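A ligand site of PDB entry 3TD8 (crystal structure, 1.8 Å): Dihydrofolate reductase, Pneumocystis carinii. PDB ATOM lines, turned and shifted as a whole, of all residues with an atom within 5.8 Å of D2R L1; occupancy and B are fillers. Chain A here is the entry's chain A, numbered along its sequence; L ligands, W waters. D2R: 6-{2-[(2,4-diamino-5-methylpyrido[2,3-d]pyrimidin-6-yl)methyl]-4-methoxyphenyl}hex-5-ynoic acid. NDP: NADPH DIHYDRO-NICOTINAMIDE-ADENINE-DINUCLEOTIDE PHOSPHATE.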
ATOM      1  N   ILE A  10      -1.855 -34.647 -33.220  1.00  0.00           N
ATOM      2  CA  ILE A  10      -2.248 -35.361 -31.961  1.00  0.00           C
ATOM      3  C   ILE A  10      -3.652 -34.816 -31.489  1.00  0.00           C
ATOM      4  O   ILE A  10      -3.944 -33.613 -31.488  1.00  0.00           O
ATOM      5  CB  ILE A  10      -1.148 -35.222 -30.867  1.00  0.00           C
ATOM      6  CG1 ILE A  10      -1.522 -36.044 -29.585  1.00  0.00           C
ATOM      7  CG2 ILE A  10      -0.778 -33.741 -30.595  1.00  0.00           C
ATOM      8  CD1 ILE A  10      -0.304 -36.259 -28.600  1.00  0.00           C
ATOM      9  N   VAL A  11      -4.524 -35.773 -31.156  1.00  0.00           N
ATOM     10  CA  VAL A  11      -5.922 -35.553 -30.904  1.00  0.00           C
ATOM     11  C   VAL A  11      -6.466 -36.698 -30.003  1.00  0.00           C
ATOM     12  O   VAL A  11      -5.997 -37.857 -30.060  1.00  0.00           O
ATOM     13  CB  VAL A  11      -6.720 -35.550 -32.254  1.00  0.00           C
ATOM     14  CG1 VAL A  11      -6.633 -36.880 -33.038  1.00  0.00           C
ATOM     15  CG2 VAL A  11      -8.180 -35.096 -32.101  1.00  0.00           C
ATOM     16  N   ALA A  12      -7.536 -36.413 -29.269  1.00  0.00           N
ATOM     17  CA  ALA A  12      -8.255 -37.428 -28.541  1.00  0.00           C
ATOM     18  C   ALA A  12      -9.661 -37.222 -29.080  1.00  0.00           C
ATOM     19  O   ALA A  12     -10.122 -36.073 -29.180  1.00  0.00           O
ATOM     20  CB  ALA A  12      -8.214 -37.175 -26.999  1.00  0.00           C
ATOM     21  N   ASN A  23     -16.266 -25.162 -26.144  1.00  0.00           N
ATOM     22  CA  ASN A  23     -14.832 -24.719 -26.134  1.00  0.00           C
ATOM     23  C   ASN A  23     -13.906 -25.390 -25.136  1.00  0.00           C
ATOM     24  O   ASN A  23     -12.943 -24.780 -24.637  1.00  0.00           O
ATOM     25  CB  ASN A  23     -14.737 -23.212 -25.990  1.00  0.00           C
ATOM     26  CG  ASN A  23     -15.446 -22.506 -27.114  1.00  0.00           C
ATOM     27  OD1 ASN A  23     -15.338 -22.908 -28.267  1.00  0.00           O
ATOM     28  ND2 ASN A  23     -16.187 -21.462 -26.781  1.00  0.00           N
ATOM     29  N   SER A  24     -14.212 -26.634 -24.811  1.00  0.00           N
ATOM     30  CA  SER A  24     -13.341 -27.429 -23.945  1.00  0.00           C
ATOM     31  C   SER A  24     -13.411 -28.890 -24.388  1.00  0.00           C
ATOM     32  O   SER A  24     -14.129 -29.205 -25.364  1.00  0.00           O
ATOM     33  CB  SER A  24     -13.780 -27.307 -22.477  1.00  0.00           C
ATOM     34  OG  SER A  24     -12.710 -27.661 -21.588  1.00  0.00           O
ATOM     35  N   LEU A  25     -12.681 -29.754 -23.689  1.00  0.00           N
ATOM     36  CA  LEU A  25     -12.777 -31.214 -23.816  1.00  0.00           C
ATOM     37  C   LEU A  25     -13.941 -31.704 -22.972  1.00  0.00           C
ATOM     38  O   LEU A  25     -14.046 -31.353 -21.791  1.00  0.00           O
ATOM     39  CB  LEU A  25     -11.475 -31.895 -23.347  1.00  0.00           C
ATOM     40  CG  LEU A  25     -10.142 -31.859 -24.116  1.00  0.00           C
ATOM     41  CD1 LEU A  25     -10.175 -31.179 -25.476  1.00  0.00           C
ATOM     42  CD2 LEU A  25      -8.967 -31.437 -23.260  1.00  0.00           C
ATOM     43  N   GLU A  32      -4.794 -39.285 -19.934  1.00  0.00           N
ATOM     44  CA  GLU A  32      -4.739 -38.848 -21.327  1.00  0.00           C
ATOM     45  C   GLU A  32      -3.988 -37.493 -21.454  1.00  0.00           C
ATOM     46  O   GLU A  32      -3.143 -37.321 -22.327  1.00  0.00           O
ATOM     47  CB  GLU A  32      -6.163 -38.738 -21.868  1.00  0.00           C
ATOM     48  CG  GLU A  32      -6.281 -38.955 -23.395  1.00  0.00           C
ATOM     49  CD  GLU A  32      -5.576 -37.879 -24.236  1.00  0.00           C
ATOM     50  OE1 GLU A  32      -5.774 -36.677 -23.978  1.00  0.00           O
ATOM     51  OE2 GLU A  32      -4.858 -38.249 -25.215  1.00  0.00           O
ATOM     52  N   ILE A  33      -4.302 -36.545 -20.568  1.00  0.00           N
ATOM     53  CA  ILE A  33      -3.502 -35.277 -20.528  1.00  0.00           C
ATOM     54  C   ILE A  33      -1.988 -35.530 -20.404  1.00  0.00           C
ATOM     55  O   ILE A  33      -1.210 -34.862 -21.096  1.00  0.00           O
ATOM     56  CB  ILE A  33      -3.986 -34.279 -19.440  1.00  0.00           C
ATOM     57  CG1 ILE A  33      -5.385 -33.730 -19.816  1.00  0.00           C
ATOM     58  CG2 ILE A  33      -2.972 -33.138 -19.313  1.00  0.00           C
ATOM     59  CD1 ILE A  33      -5.356 -32.620 -20.846  1.00  0.00           C
ATOM     60  N   TYR A  35      -0.284 -38.182 -21.358  1.00  0.00           N
ATOM     61  CA  TYR A  35       0.238 -38.734 -22.622  1.00  0.00           C
ATOM     62  C   TYR A  35       0.480 -37.594 -23.626  1.00  0.00           C
ATOM     63  O   TYR A  35       1.559 -37.476 -24.246  1.00  0.00           O
ATOM     64  CB  TYR A  35      -0.767 -39.716 -23.196  1.00  0.00           C
ATOM     65  CG  TYR A  35      -0.406 -40.304 -24.546  1.00  0.00           C
ATOM     66  CD1 TYR A  35       0.508 -41.340 -24.633  1.00  0.00           C
ATOM     67  CD2 TYR A  35      -1.013 -39.849 -25.736  1.00  0.00           C
ATOM     68  CE1 TYR A  35       0.806 -41.954 -25.835  1.00  0.00           C
ATOM     69  CE2 TYR A  35      -0.696 -40.438 -26.973  1.00  0.00           C
ATOM     70  CZ  TYR A  35       0.213 -41.497 -27.007  1.00  0.00           C
ATOM     71  OH  TYR A  35       0.558 -42.129 -28.203  1.00  0.00           O
ATOM     72  N   PHE A  36      -0.492 -36.739 -23.703  1.00  0.00           N
ATOM     73  CA  PHE A  36      -0.384 -35.591 -24.571  1.00  0.00           C
ATOM     74  C   PHE A  36       0.866 -34.779 -24.184  1.00  0.00           C
ATOM     75  O   PHE A  36       1.651 -34.452 -25.021  1.00  0.00           O
ATOM     76  CB  PHE A  36      -1.573 -34.728 -24.439  1.00  0.00           C
ATOM     77  CG  PHE A  36      -1.393 -33.399 -25.104  1.00  0.00           C
ATOM     78  CD1 PHE A  36      -1.576 -33.262 -26.501  1.00  0.00           C
ATOM     79  CD2 PHE A  36      -0.972 -32.305 -24.377  1.00  0.00           C
ATOM     80  CE1 PHE A  36      -1.389 -32.011 -27.128  1.00  0.00           C
ATOM     81  CE2 PHE A  36      -0.760 -31.058 -24.982  1.00  0.00           C
ATOM     82  CZ  PHE A  36      -0.969 -30.916 -26.364  1.00  0.00           C
ATOM     83  N   LYS A  37       1.043 -34.458 -22.879  1.00  0.00           N
ATOM     84  CA  LYS A  37       2.170 -33.630 -22.428  1.00  0.00           C
ATOM     85  C   LYS A  37       3.432 -34.340 -22.786  1.00  0.00           C
ATOM     86  O   LYS A  37       4.340 -33.760 -23.349  1.00  0.00           O
ATOM     87  CB  LYS A  37       2.088 -33.406 -20.884  1.00  0.00           C
ATOM     88  CG  LYS A  37       3.223 -32.604 -20.260  1.00  0.00           C
ATOM     89  CD  LYS A  37       2.849 -32.285 -18.812  1.00  0.00           C
ATOM     90  CE  LYS A  37       3.768 -31.240 -18.163  1.00  0.00           C
ATOM     91  NZ  LYS A  37       5.214 -31.576 -18.361  1.00  0.00           N
ATOM     92  N   THR A  40       4.216 -34.702 -26.902  1.00  0.00           N
ATOM     93  CA  THR A  40       4.521 -33.429 -27.553  1.00  0.00           C
ATOM     94  C   THR A  40       5.811 -32.852 -26.999  1.00  0.00           C
ATOM     95  O   THR A  40       6.415 -32.074 -27.687  1.00  0.00           O
ATOM     96  CB  THR A  40       3.405 -32.348 -27.484  1.00  0.00           C
ATOM     97  OG1 THR A  40       3.113 -32.005 -26.135  1.00  0.00           O
ATOM     98  CG2 THR A  40       2.077 -32.860 -28.171  1.00  0.00           C
ATOM     99  N   LYS A  60      -8.671 -20.637 -31.314  1.00  0.00           N
ATOM    100  CA  LYS A  60      -9.738 -21.086 -30.386  1.00  0.00           C
ATOM    101  C   LYS A  60      -9.231 -22.064 -29.320  1.00  0.00           C
ATOM    102  O   LYS A  60      -9.523 -21.889 -28.158  1.00  0.00           O
ATOM    103  CB  LYS A  60     -11.012 -21.583 -31.105  1.00  0.00           C
ATOM    104  CG  LYS A  60     -11.616 -20.439 -31.905  1.00  0.00           C
ATOM    105  CD  LYS A  60     -12.825 -20.757 -32.766  1.00  0.00           C
ATOM    106  CE  LYS A  60     -14.039 -19.991 -32.249  1.00  0.00           C
ATOM    107  NZ  LYS A  60     -15.051 -19.830 -33.339  1.00  0.00           N
ATOM    108  N   THR A  61      -8.431 -23.046 -29.739  1.00  0.00           N
ATOM    109  CA  THR A  61      -7.720 -23.954 -28.850  1.00  0.00           C
ATOM    110  C   THR A  61      -6.803 -23.173 -27.874  1.00  0.00           C
ATOM    111  O   THR A  61      -6.768 -23.469 -26.672  1.00  0.00           O
ATOM    112  CB  THR A  61      -6.923 -24.973 -29.698  1.00  0.00           C
ATOM    113  OG1 THR A  61      -7.899 -25.790 -30.392  1.00  0.00           O
ATOM    114  CG2 THR A  61      -5.926 -25.763 -28.868  1.00  0.00           C
ATOM    115  N   SER A  64      -8.923 -21.777 -25.178  1.00  0.00           N
ATOM    116  CA  SER A  64      -9.515 -22.887 -24.380  1.00  0.00           C
ATOM    117  C   SER A  64      -8.596 -23.463 -23.299  1.00  0.00           C
ATOM    118  O   SER A  64      -9.064 -24.009 -22.317  1.00  0.00           O
ATOM    119  CB  SER A  64      -9.921 -24.042 -25.287  1.00  0.00           C
ATOM    120  OG  SER A  64     -10.979 -23.675 -26.132  1.00  0.00           O
ATOM    121  N   ILE A  65      -7.295 -23.341 -23.478  1.00  0.00           N
ATOM    122  CA  ILE A  65      -6.370 -23.926 -22.519  1.00  0.00           C
ATOM    123  C   ILE A  65      -6.448 -23.101 -21.220  1.00  0.00           C
ATOM    124  O   ILE A  65      -6.342 -21.861 -21.301  1.00  0.00           O
ATOM    125  CB  ILE A  65      -4.938 -24.010 -23.098  1.00  0.00           C
ATOM    126  CG1 ILE A  65      -4.924 -24.951 -24.350  1.00  0.00           C
ATOM    127  CG2 ILE A  65      -3.985 -24.488 -22.034  1.00  0.00           C
ATOM    128  CD1 ILE A  65      -3.588 -25.122 -25.053  1.00  0.00           C
ATOM    129  N   PRO A  66      -6.674 -23.774 -20.049  1.00  0.00           N
ATOM    130  CA  PRO A  66      -6.675 -23.007 -18.783  1.00  0.00           C
ATOM    131  C   PRO A  66      -5.398 -22.185 -18.682  1.00  0.00           C
ATOM    132  O   PRO A  66      -4.322 -22.607 -19.130  1.00  0.00           O
ATOM    133  CB  PRO A  66      -6.722 -24.084 -17.709  1.00  0.00           C
ATOM    134  CG  PRO A  66      -7.408 -25.229 -18.364  1.00  0.00           C
ATOM    135  CD  PRO A  66      -6.865 -25.206 -19.785  1.00  0.00           C
ATOM    136  N   PHE A  69      -1.887 -23.269 -17.730  1.00  0.00           N
ATOM    137  CA  PHE A  69      -1.122 -24.109 -18.663  1.00  0.00           C
ATOM    138  C   PHE A  69      -0.554 -23.410 -19.929  1.00  0.00           C
ATOM    139  O   PHE A  69       0.223 -24.020 -20.649  1.00  0.00           O
ATOM    140  CB  PHE A  69      -1.944 -25.334 -19.049  1.00  0.00           C
ATOM    141  CG  PHE A  69      -2.433 -26.126 -17.864  1.00  0.00           C
ATOM    142  CD1 PHE A  69      -1.526 -26.823 -17.052  1.00  0.00           C
ATOM    143  CD2 PHE A  69      -3.786 -26.163 -17.539  1.00  0.00           C
ATOM    144  CE1 PHE A  69      -1.961 -27.549 -15.963  1.00  0.00           C
ATOM    145  CE2 PHE A  69      -4.228 -26.885 -16.445  1.00  0.00           C
ATOM    146  CZ  PHE A  69      -3.310 -27.587 -15.651  1.00  0.00           C
ATOM    147  N   LEU A  72       2.140 -23.746 -23.386  1.00  0.00           N
ATOM    148  CA  LEU A  72       2.452 -25.099 -23.008  1.00  0.00           C
ATOM    149  C   LEU A  72       3.956 -25.185 -22.786  1.00  0.00           C
ATOM    150  O   LEU A  72       4.747 -24.964 -23.721  1.00  0.00           O
ATOM    151  CB  LEU A  72       2.018 -26.108 -24.105  1.00  0.00           C
ATOM    152  CG  LEU A  72       0.505 -26.327 -24.290  1.00  0.00           C
ATOM    153  CD1 LEU A  72       0.267 -27.341 -25.412  1.00  0.00           C
ATOM    154  CD2 LEU A  72      -0.182 -26.774 -22.984  1.00  0.00           C
ATOM    155  N   LYS A  73       4.343 -25.515 -21.553  1.00  0.00           N
ATOM    156  CA  LYS A  73       5.757 -25.459 -21.112  1.00  0.00           C
ATOM    157  C   LYS A  73       6.644 -26.399 -21.837  1.00  0.00           C
ATOM    158  O   LYS A  73       6.267 -27.556 -22.108  1.00  0.00           O
ATOM    159  CB  LYS A  73       5.885 -25.746 -19.603  1.00  0.00           C
ATOM    160  CG  LYS A  73       5.602 -24.544 -18.737  1.00  0.00           C
ATOM    161  CD  LYS A  73       5.659 -24.890 -17.260  1.00  0.00           C
ATOM    162  CE  LYS A  73       5.617 -23.601 -16.454  1.00  0.00           C
ATOM    163  NZ  LYS A  73       4.717 -23.707 -15.265  1.00  0.00           N
ATOM    164  N   ARG A  75       7.758 -26.292 -24.832  1.00  0.00           N
ATOM    165  CA  ARG A  75       7.547 -26.539 -26.233  1.00  0.00           C
ATOM    166  C   ARG A  75       7.460 -25.174 -26.865  1.00  0.00           C
ATOM    167  O   ARG A  75       6.967 -24.218 -26.229  1.00  0.00           O
ATOM    168  CB  ARG A  75       6.258 -27.324 -26.443  1.00  0.00           C
ATOM    169  CG  ARG A  75       6.315 -28.809 -26.106  1.00  0.00           C
ATOM    170  CD  ARG A  75       4.945 -29.275 -25.528  1.00  0.00           C
ATOM    171  NE  ARG A  75       4.743 -28.765 -24.152  1.00  0.00           N
ATOM    172  CZ  ARG A  75       3.734 -29.113 -23.367  1.00  0.00           C
ATOM    173  NH1 ARG A  75       2.807 -29.948 -23.835  1.00  0.00           N
ATOM    174  NH2 ARG A  75       3.631 -28.648 -22.124  1.00  0.00           N
ATOM    175  N   VAL A 122       0.646 -30.620 -34.553  1.00  0.00           N
ATOM    176  CA  VAL A 122      -0.572 -29.842 -34.704  1.00  0.00           C
ATOM    177  C   VAL A 122      -1.478 -30.355 -33.583  1.00  0.00           C
ATOM    178  O   VAL A 122      -1.827 -31.568 -33.564  1.00  0.00           O
ATOM    179  CB  VAL A 122      -1.259 -30.038 -36.094  1.00  0.00           C
ATOM    180  CG1 VAL A 122      -2.616 -29.223 -36.165  1.00  0.00           C
ATOM    181  CG2 VAL A 122      -0.306 -29.578 -37.219  1.00  0.00           C
ATOM    182  N   ILE A 123      -1.949 -29.462 -32.701  1.00  0.00           N
ATOM    183  CA  ILE A 123      -2.616 -29.978 -31.464  1.00  0.00           C
ATOM    184  C   ILE A 123      -4.065 -29.560 -31.421  1.00  0.00           C
ATOM    185  O   ILE A 123      -4.716 -29.802 -30.420  1.00  0.00           O
ATOM    186  CB  ILE A 123      -1.894 -29.502 -30.189  1.00  0.00           C
ATOM    187  CG1 ILE A 123      -1.956 -27.943 -30.045  1.00  0.00           C
ATOM    188  CG2 ILE A 123      -0.464 -30.062 -30.214  1.00  0.00           C
ATOM    189  CD1 ILE A 123      -1.692 -27.459 -28.598  1.00  0.00           C
ATOM    190  N   GLY A 124      -4.544 -28.910 -32.476  1.00  0.00           N
ATOM    191  CA  GLY A 124      -5.989 -28.617 -32.595  1.00  0.00           C
ATOM    192  C   GLY A 124      -6.204 -27.164 -32.879  1.00  0.00           C
ATOM    193  O   GLY A 124      -5.220 -26.442 -33.000  1.00  0.00           O
ATOM    194  N   TYR A 129      -6.816 -28.791 -37.635  1.00  0.00           N
ATOM    195  CA  TYR A 129      -6.756 -30.150 -37.998  1.00  0.00           C
ATOM    196  C   TYR A 129      -7.049 -30.328 -39.499  1.00  0.00           C
ATOM    197  O   TYR A 129      -6.354 -31.088 -40.209  1.00  0.00           O
ATOM    198  CB  TYR A 129      -7.759 -31.035 -37.206  1.00  0.00           C
ATOM    199  CG  TYR A 129      -7.299 -31.349 -35.781  1.00  0.00           C
ATOM    200  CD1 TYR A 129      -5.951 -31.542 -35.477  1.00  0.00           C
ATOM    201  CD2 TYR A 129      -8.219 -31.458 -34.758  1.00  0.00           C
ATOM    202  CE1 TYR A 129      -5.512 -31.871 -34.187  1.00  0.00           C
ATOM    203  CE2 TYR A 129      -7.788 -31.746 -33.496  1.00  0.00           C
ATOM    204  CZ  TYR A 129      -6.448 -31.909 -33.190  1.00  0.00           C
ATOM    205  OH  TYR A 129      -6.144 -32.215 -31.862  1.00  0.00           O
ATOM    206  N   MET A 142      -1.547 -39.164 -33.932  1.00  0.00           N
ATOM    207  CA  MET A 142      -1.385 -39.816 -32.647  1.00  0.00           C
ATOM    208  C   MET A 142      -2.778 -39.671 -32.124  1.00  0.00           C
ATOM    209  O   MET A 142      -3.178 -38.561 -31.744  1.00  0.00           O
ATOM    210  CB  MET A 142      -0.464 -38.997 -31.777  1.00  0.00           C
ATOM    211  CG  MET A 142       0.991 -38.871 -32.329  1.00  0.00           C
ATOM    212  SD  MET A 142       1.686 -40.458 -32.828  1.00  0.00           S
ATOM    213  CE  MET A 142       1.963 -41.369 -31.363  1.00  0.00           C
ATOM    214  N   THR A 144      -5.960 -40.539 -29.691  1.00  0.00           N
ATOM    215  CA  THR A 144      -6.497 -41.228 -28.529  1.00  0.00           C
ATOM    216  C   THR A 144      -7.990 -41.528 -28.751  1.00  0.00           C
ATOM    217  O   THR A 144      -8.769 -40.626 -28.903  1.00  0.00           O
ATOM    218  CB  THR A 144      -6.261 -40.400 -27.226  1.00  0.00           C
ATOM    219  OG1 THR A 144      -4.845 -40.192 -27.035  1.00  0.00           O
ATOM    220  CG2 THR A 144      -6.808 -41.237 -26.065  1.00  0.00           C
HETATM  221  N1  D2R L   1      -4.476 -34.218 -28.014  1.00  0.00           N
HETATM  222  C2  D2R L   1      -4.730 -35.090 -27.027  1.00  0.00           C
HETATM  223  N3  D2R L   1      -5.035 -34.686 -25.790  1.00  0.00           N
HETATM  224  C4  D2R L   1      -5.037 -33.384 -25.509  1.00  0.00           C
HETATM  225  C5  D2R L   1      -4.821 -32.393 -26.518  1.00  0.00           C
HETATM  226  C6  D2R L   1      -4.558 -32.896 -27.850  1.00  0.00           C
HETATM  227  CAA D2R L   1      -9.277 -26.976 -25.908  1.00  0.00           C
HETATM  228  CAB D2R L   1      -4.617 -29.805 -27.104  1.00  0.00           C
HETATM  229  NAC D2R L   1      -4.685 -36.421 -27.258  1.00  0.00           N
HETATM  230  NAD D2R L   1      -4.329 -32.089 -28.896  1.00  0.00           N
HETATM  231  OAE D2R L   1       0.421 -30.252 -21.918  1.00  0.00           O
HETATM  232  OAF D2R L   1       1.466 -29.096 -20.351  1.00  0.00           O
HETATM  233  CAG D2R L   1      -4.463 -29.079 -20.764  1.00  0.00           C
HETATM  234  CAH D2R L   1      -5.419 -28.820 -21.463  1.00  0.00           C
HETATM  235  CAI D2R L   1      -8.861 -27.821 -22.536  1.00  0.00           C
HETATM  236  CAJ D2R L   1      -7.762 -28.095 -21.714  1.00  0.00           C
HETATM  237  CAK D2R L   1      -5.327 -31.728 -23.924  1.00  0.00           C
HETATM  238  CAL D2R L   1      -7.510 -28.424 -24.500  1.00  0.00           C
HETATM  239  CAM D2R L   1      -3.340 -29.362 -19.840  1.00  0.00           C
HETATM  240  CAN D2R L   1      -2.147 -29.767 -20.685  1.00  0.00           C
HETATM  241  CAO D2R L   1      -0.832 -29.436 -19.997  1.00  0.00           C
HETATM  242  CAP D2R L   1      -5.150 -29.192 -24.306  1.00  0.00           C
HETATM  243  NAQ D2R L   1      -5.299 -33.033 -24.242  1.00  0.00           N
HETATM  244  OAT D2R L   1      -9.764 -27.707 -24.772  1.00  0.00           O
HETATM  245  CAU D2R L   1       0.440 -29.607 -20.833  1.00  0.00           C
HETATM  246  CAX D2R L   1      -4.841 -31.013 -26.155  1.00  0.00           C
HETATM  247  CAY D2R L   1      -8.717 -27.973 -23.934  1.00  0.00           C
HETATM  248  CAZ D2R L   1      -6.554 -28.535 -22.288  1.00  0.00           C
HETATM  249  CBA D2R L   1      -5.119 -30.678 -24.817  1.00  0.00           C
HETATM  250  CBB D2R L   1      -6.432 -28.732 -23.679  1.00  0.00           C
HETATM  251  PA  NDP L   2      -9.299 -23.914 -33.657  1.00  0.00           P
HETATM  252  O1A NDP L   2      -8.582 -24.087 -32.374  1.00  0.00           O
HETATM  253  O2A NDP L   2      -8.852 -24.558 -34.951  1.00  0.00           O
HETATM  254  O5B NDP L   2      -9.246 -22.347 -33.924  1.00  0.00           O
HETATM  255  C5B NDP L   2      -9.873 -21.751 -35.090  1.00  0.00           C
HETATM  256  C4B NDP L   2      -9.232 -20.469 -35.433  1.00  0.00           C
HETATM  257  O4B NDP L   2      -7.759 -20.601 -35.573  1.00  0.00           O
HETATM  258  C3B NDP L   2      -9.700 -19.884 -36.713  1.00  0.00           C
HETATM  259  O3B NDP L   2     -10.801 -18.973 -36.512  1.00  0.00           O
HETATM  260  C2B NDP L   2      -8.447 -19.049 -37.072  1.00  0.00           C
HETATM  261  O2B NDP L   2      -8.254 -17.936 -36.183  1.00  0.00           O
HETATM  262  C1B NDP L   2      -7.313 -20.007 -36.748  1.00  0.00           C
HETATM  263  N9A NDP L   2      -7.097 -21.052 -37.771  1.00  0.00           N
HETATM  264  C8A NDP L   2      -7.384 -22.366 -37.711  1.00  0.00           C
HETATM  265  N7A NDP L   2      -6.981 -22.977 -38.881  1.00  0.00           N
HETATM  266  C5A NDP L   2      -6.416 -22.018 -39.626  1.00  0.00           C
HETATM  267  C6A NDP L   2      -5.825 -22.033 -40.885  1.00  0.00           C
HETATM  268  N6A NDP L   2      -5.751 -23.181 -41.610  1.00  0.00           N
HETATM  269  N1A NDP L   2      -5.331 -20.855 -41.334  1.00  0.00           N
HETATM  270  C2A NDP L   2      -5.428 -19.715 -40.635  1.00  0.00           C
HETATM  271  N3A NDP L   2      -5.986 -19.659 -39.424  1.00  0.00           N
HETATM  272  C4A NDP L   2      -6.517 -20.793 -38.930  1.00  0.00           C
HETATM  273  O3  NDP L   2     -10.861 -24.122 -33.408  1.00  0.00           O
HETATM  274  PN  NDP L   2     -11.981 -25.055 -33.737  1.00  0.00           P
HETATM  275  O1N NDP L   2     -12.034 -25.484 -35.160  1.00  0.00           O
HETATM  276  O2N NDP L   2     -13.216 -24.370 -33.238  1.00  0.00           O
HETATM  277  O5D NDP L   2     -11.757 -26.184 -32.694  1.00  0.00           O
HETATM  278  C5D NDP L   2     -11.697 -25.833 -31.231  1.00  0.00           C
HETATM  279  C4D NDP L   2     -12.408 -26.971 -30.503  1.00  0.00           C
HETATM  280  O4D NDP L   2     -11.479 -28.097 -30.627  1.00  0.00           O
HETATM  281  C3D NDP L   2     -12.783 -26.938 -29.003  1.00  0.00           C
HETATM  282  O3D NDP L   2     -13.924 -27.839 -28.777  1.00  0.00           O
HETATM  283  C2D NDP L   2     -11.575 -27.521 -28.363  1.00  0.00           C
HETATM  284  O2D NDP L   2     -11.883 -27.926 -27.013  1.00  0.00           O
HETATM  285  C1D NDP L   2     -11.431 -28.751 -29.289  1.00  0.00           C
HETATM  286  N1N NDP L   2     -10.137 -29.429 -29.233  1.00  0.00           N
HETATM  287  C2N NDP L   2     -10.046 -30.813 -28.993  1.00  0.00           C
HETATM  288  C3N NDP L   2      -8.825 -31.468 -28.964  1.00  0.00           C
HETATM  289  C7N NDP L   2      -8.725 -32.964 -28.733  1.00  0.00           C
HETATM  290  O7N NDP L   2      -7.662 -33.531 -28.715  1.00  0.00           O
HETATM  291  N7N NDP L   2      -9.846 -33.632 -28.424  1.00  0.00           N
HETATM  292  C4N NDP L   2      -7.522 -30.671 -29.199  1.00  0.00           C
HETATM  293  C5N NDP L   2      -7.728 -29.290 -29.327  1.00  0.00           C
HETATM  294  C6N NDP L   2      -8.973 -28.677 -29.394  1.00  0.00           C
HETATM  295  P2B NDP L   2      -8.651 -16.386 -36.581  1.00  0.00           P
HETATM  296  O1X NDP L   2      -8.106 -16.001 -37.922  1.00  0.00           O
HETATM  297  O2X NDP L   2      -7.874 -15.633 -35.409  1.00  0.00           O
HETATM  298  O3X NDP L   2     -10.233 -16.567 -36.405  1.00  0.00           O
HETATM  299  O   HOH W   1      -7.804 -35.100 -23.210  1.00  0.00           O
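OAT of D2R L1 sits close to O2D of NDP L2, at 3.1 Å.
The side-chain hydroxyl (OG1) of Thr 144 sits at hydrogen-bond distance from the side-chain carboxylate (OE2) of Glu 32 (2.7 Å).
NE of Arg 75 is in hydrogen-bond range of O of Lys 73 (2.8 Å).
O of Ile 10 is in hydrogen-bond range of OH of Tyr 129 (2.6 Å).
O of Phe 36 sits at hydrogen-bond distance from OG1 of Thr 40.
The backbone carbonyl oxygen (O) of Val 11 lies within hydrogen-bond range of the backbone NH (N) of Thr 144.
O of Asn 23 sits at hydrogen-bond distance from OG of Ser 64, at 2.7 Å.
The guanidinium group of Arg 75 is in hydrogen-bond range of the side-chain hydroxyl of Thr 40 (3.1 Å).
N of Val 11 lies within hydrogen-bond range of O of Met 142, at 3.2 Å.
OH of Tyr 129 is in hydrogen-bond range of NAD of D2R L1, 3.5 Å away.
The backbone carbonyl oxygen of Val 11 lies close to a nitrogen (NAC) of D2R L1 (3.4 Å).
OE2 of Glu 32 lies within hydrogen-bond range of NAC of D2R L1, at 2.7 Å.
The backbone NH of Ser 24 lies close to an oxygen (O2D) of NDP L2, 3.5 Å away.
The backbone carbonyl oxygen of Ser 24 lies within hydrogen-bond range of an oxygen (O2D) of NDP L2 (3.1 Å).
The backbone NH (N) of Thr 61 lies within hydrogen-bond range of an oxygen (O1A) of NDP L2, 2.8 Å away.
The backbone carbonyl oxygen (O) of Ile 10 is in hydrogen-bond range of a nitrogen (NAD) of D2R L1, 3.0 Å away.
The backbone NH of Ala 12 sits at hydrogen-bond distance from an oxygen (O7N) of NDP L2 (2.9 Å).
The side-chain hydroxyl (OG1) of Thr 61 sits at hydrogen-bond distance from an oxygen (O1A) of NDP L2 (2.7 Å).
NH2 of Arg 75 is in salt-bridge range of OAF of D2R L1 (2.8 Å).
The backbone carbonyl oxygen (O) of Ala 12 lies within hydrogen-bond range of a nitrogen (N7N) of NDP L2, at 2.6 Å.
The backbone carbonyl oxygen (O) of Ile 123 is in hydrogen-bond range of a nitrogen (NAD) of D2R L1, 2.8 Å away.
The backbone NH (N) of Lys 60 sits at hydrogen-bond distance from an oxygen (O5B) of NDP L2, at 3.2 Å.
N of Ala 12 lies close to NAC of D2R L1.
Residues that only touch D2R L1: Ser 64 (3.1 Å), Ile 33 (3.2 Å), Phe 36 (3.3 Å), Leu 25 (3.5 Å), Pro 66 (3.6 Å), Leu 72 (3.6 Å), Ser 24 (3.7 Å), Lys 37 (3.7 Å), Thr 144 (3.8 Å) and Phe 69 (3.9 Å).
Hydrophobic or aromatic side chains that line D2R L1: Ile 10, Ala 12, Leu 25, Ile 33, Phe 36, Pro 66, Phe 69, Leu 72 and Ile 123.
17 residues have an atom within 4 Å of D2R L1: Ile 10, Val 11, Ala 12, Ser 24, Leu 25, Glu 32, Ile 33, Phe 36, Lys 37, Ser 64, Pro 66, Phe 69, Leu 72, Arg 75, Ile 123, Tyr 129 and Thr 144.
The nearest printed residue that does not touch D2R L1 is Ile 65 (4.1 Å).
Water W1 bridges the side-chain carboxylate of Glu 32 (2.7 Å) and a nitrogen (NAQ) of D2R L1 (3.4 Å).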
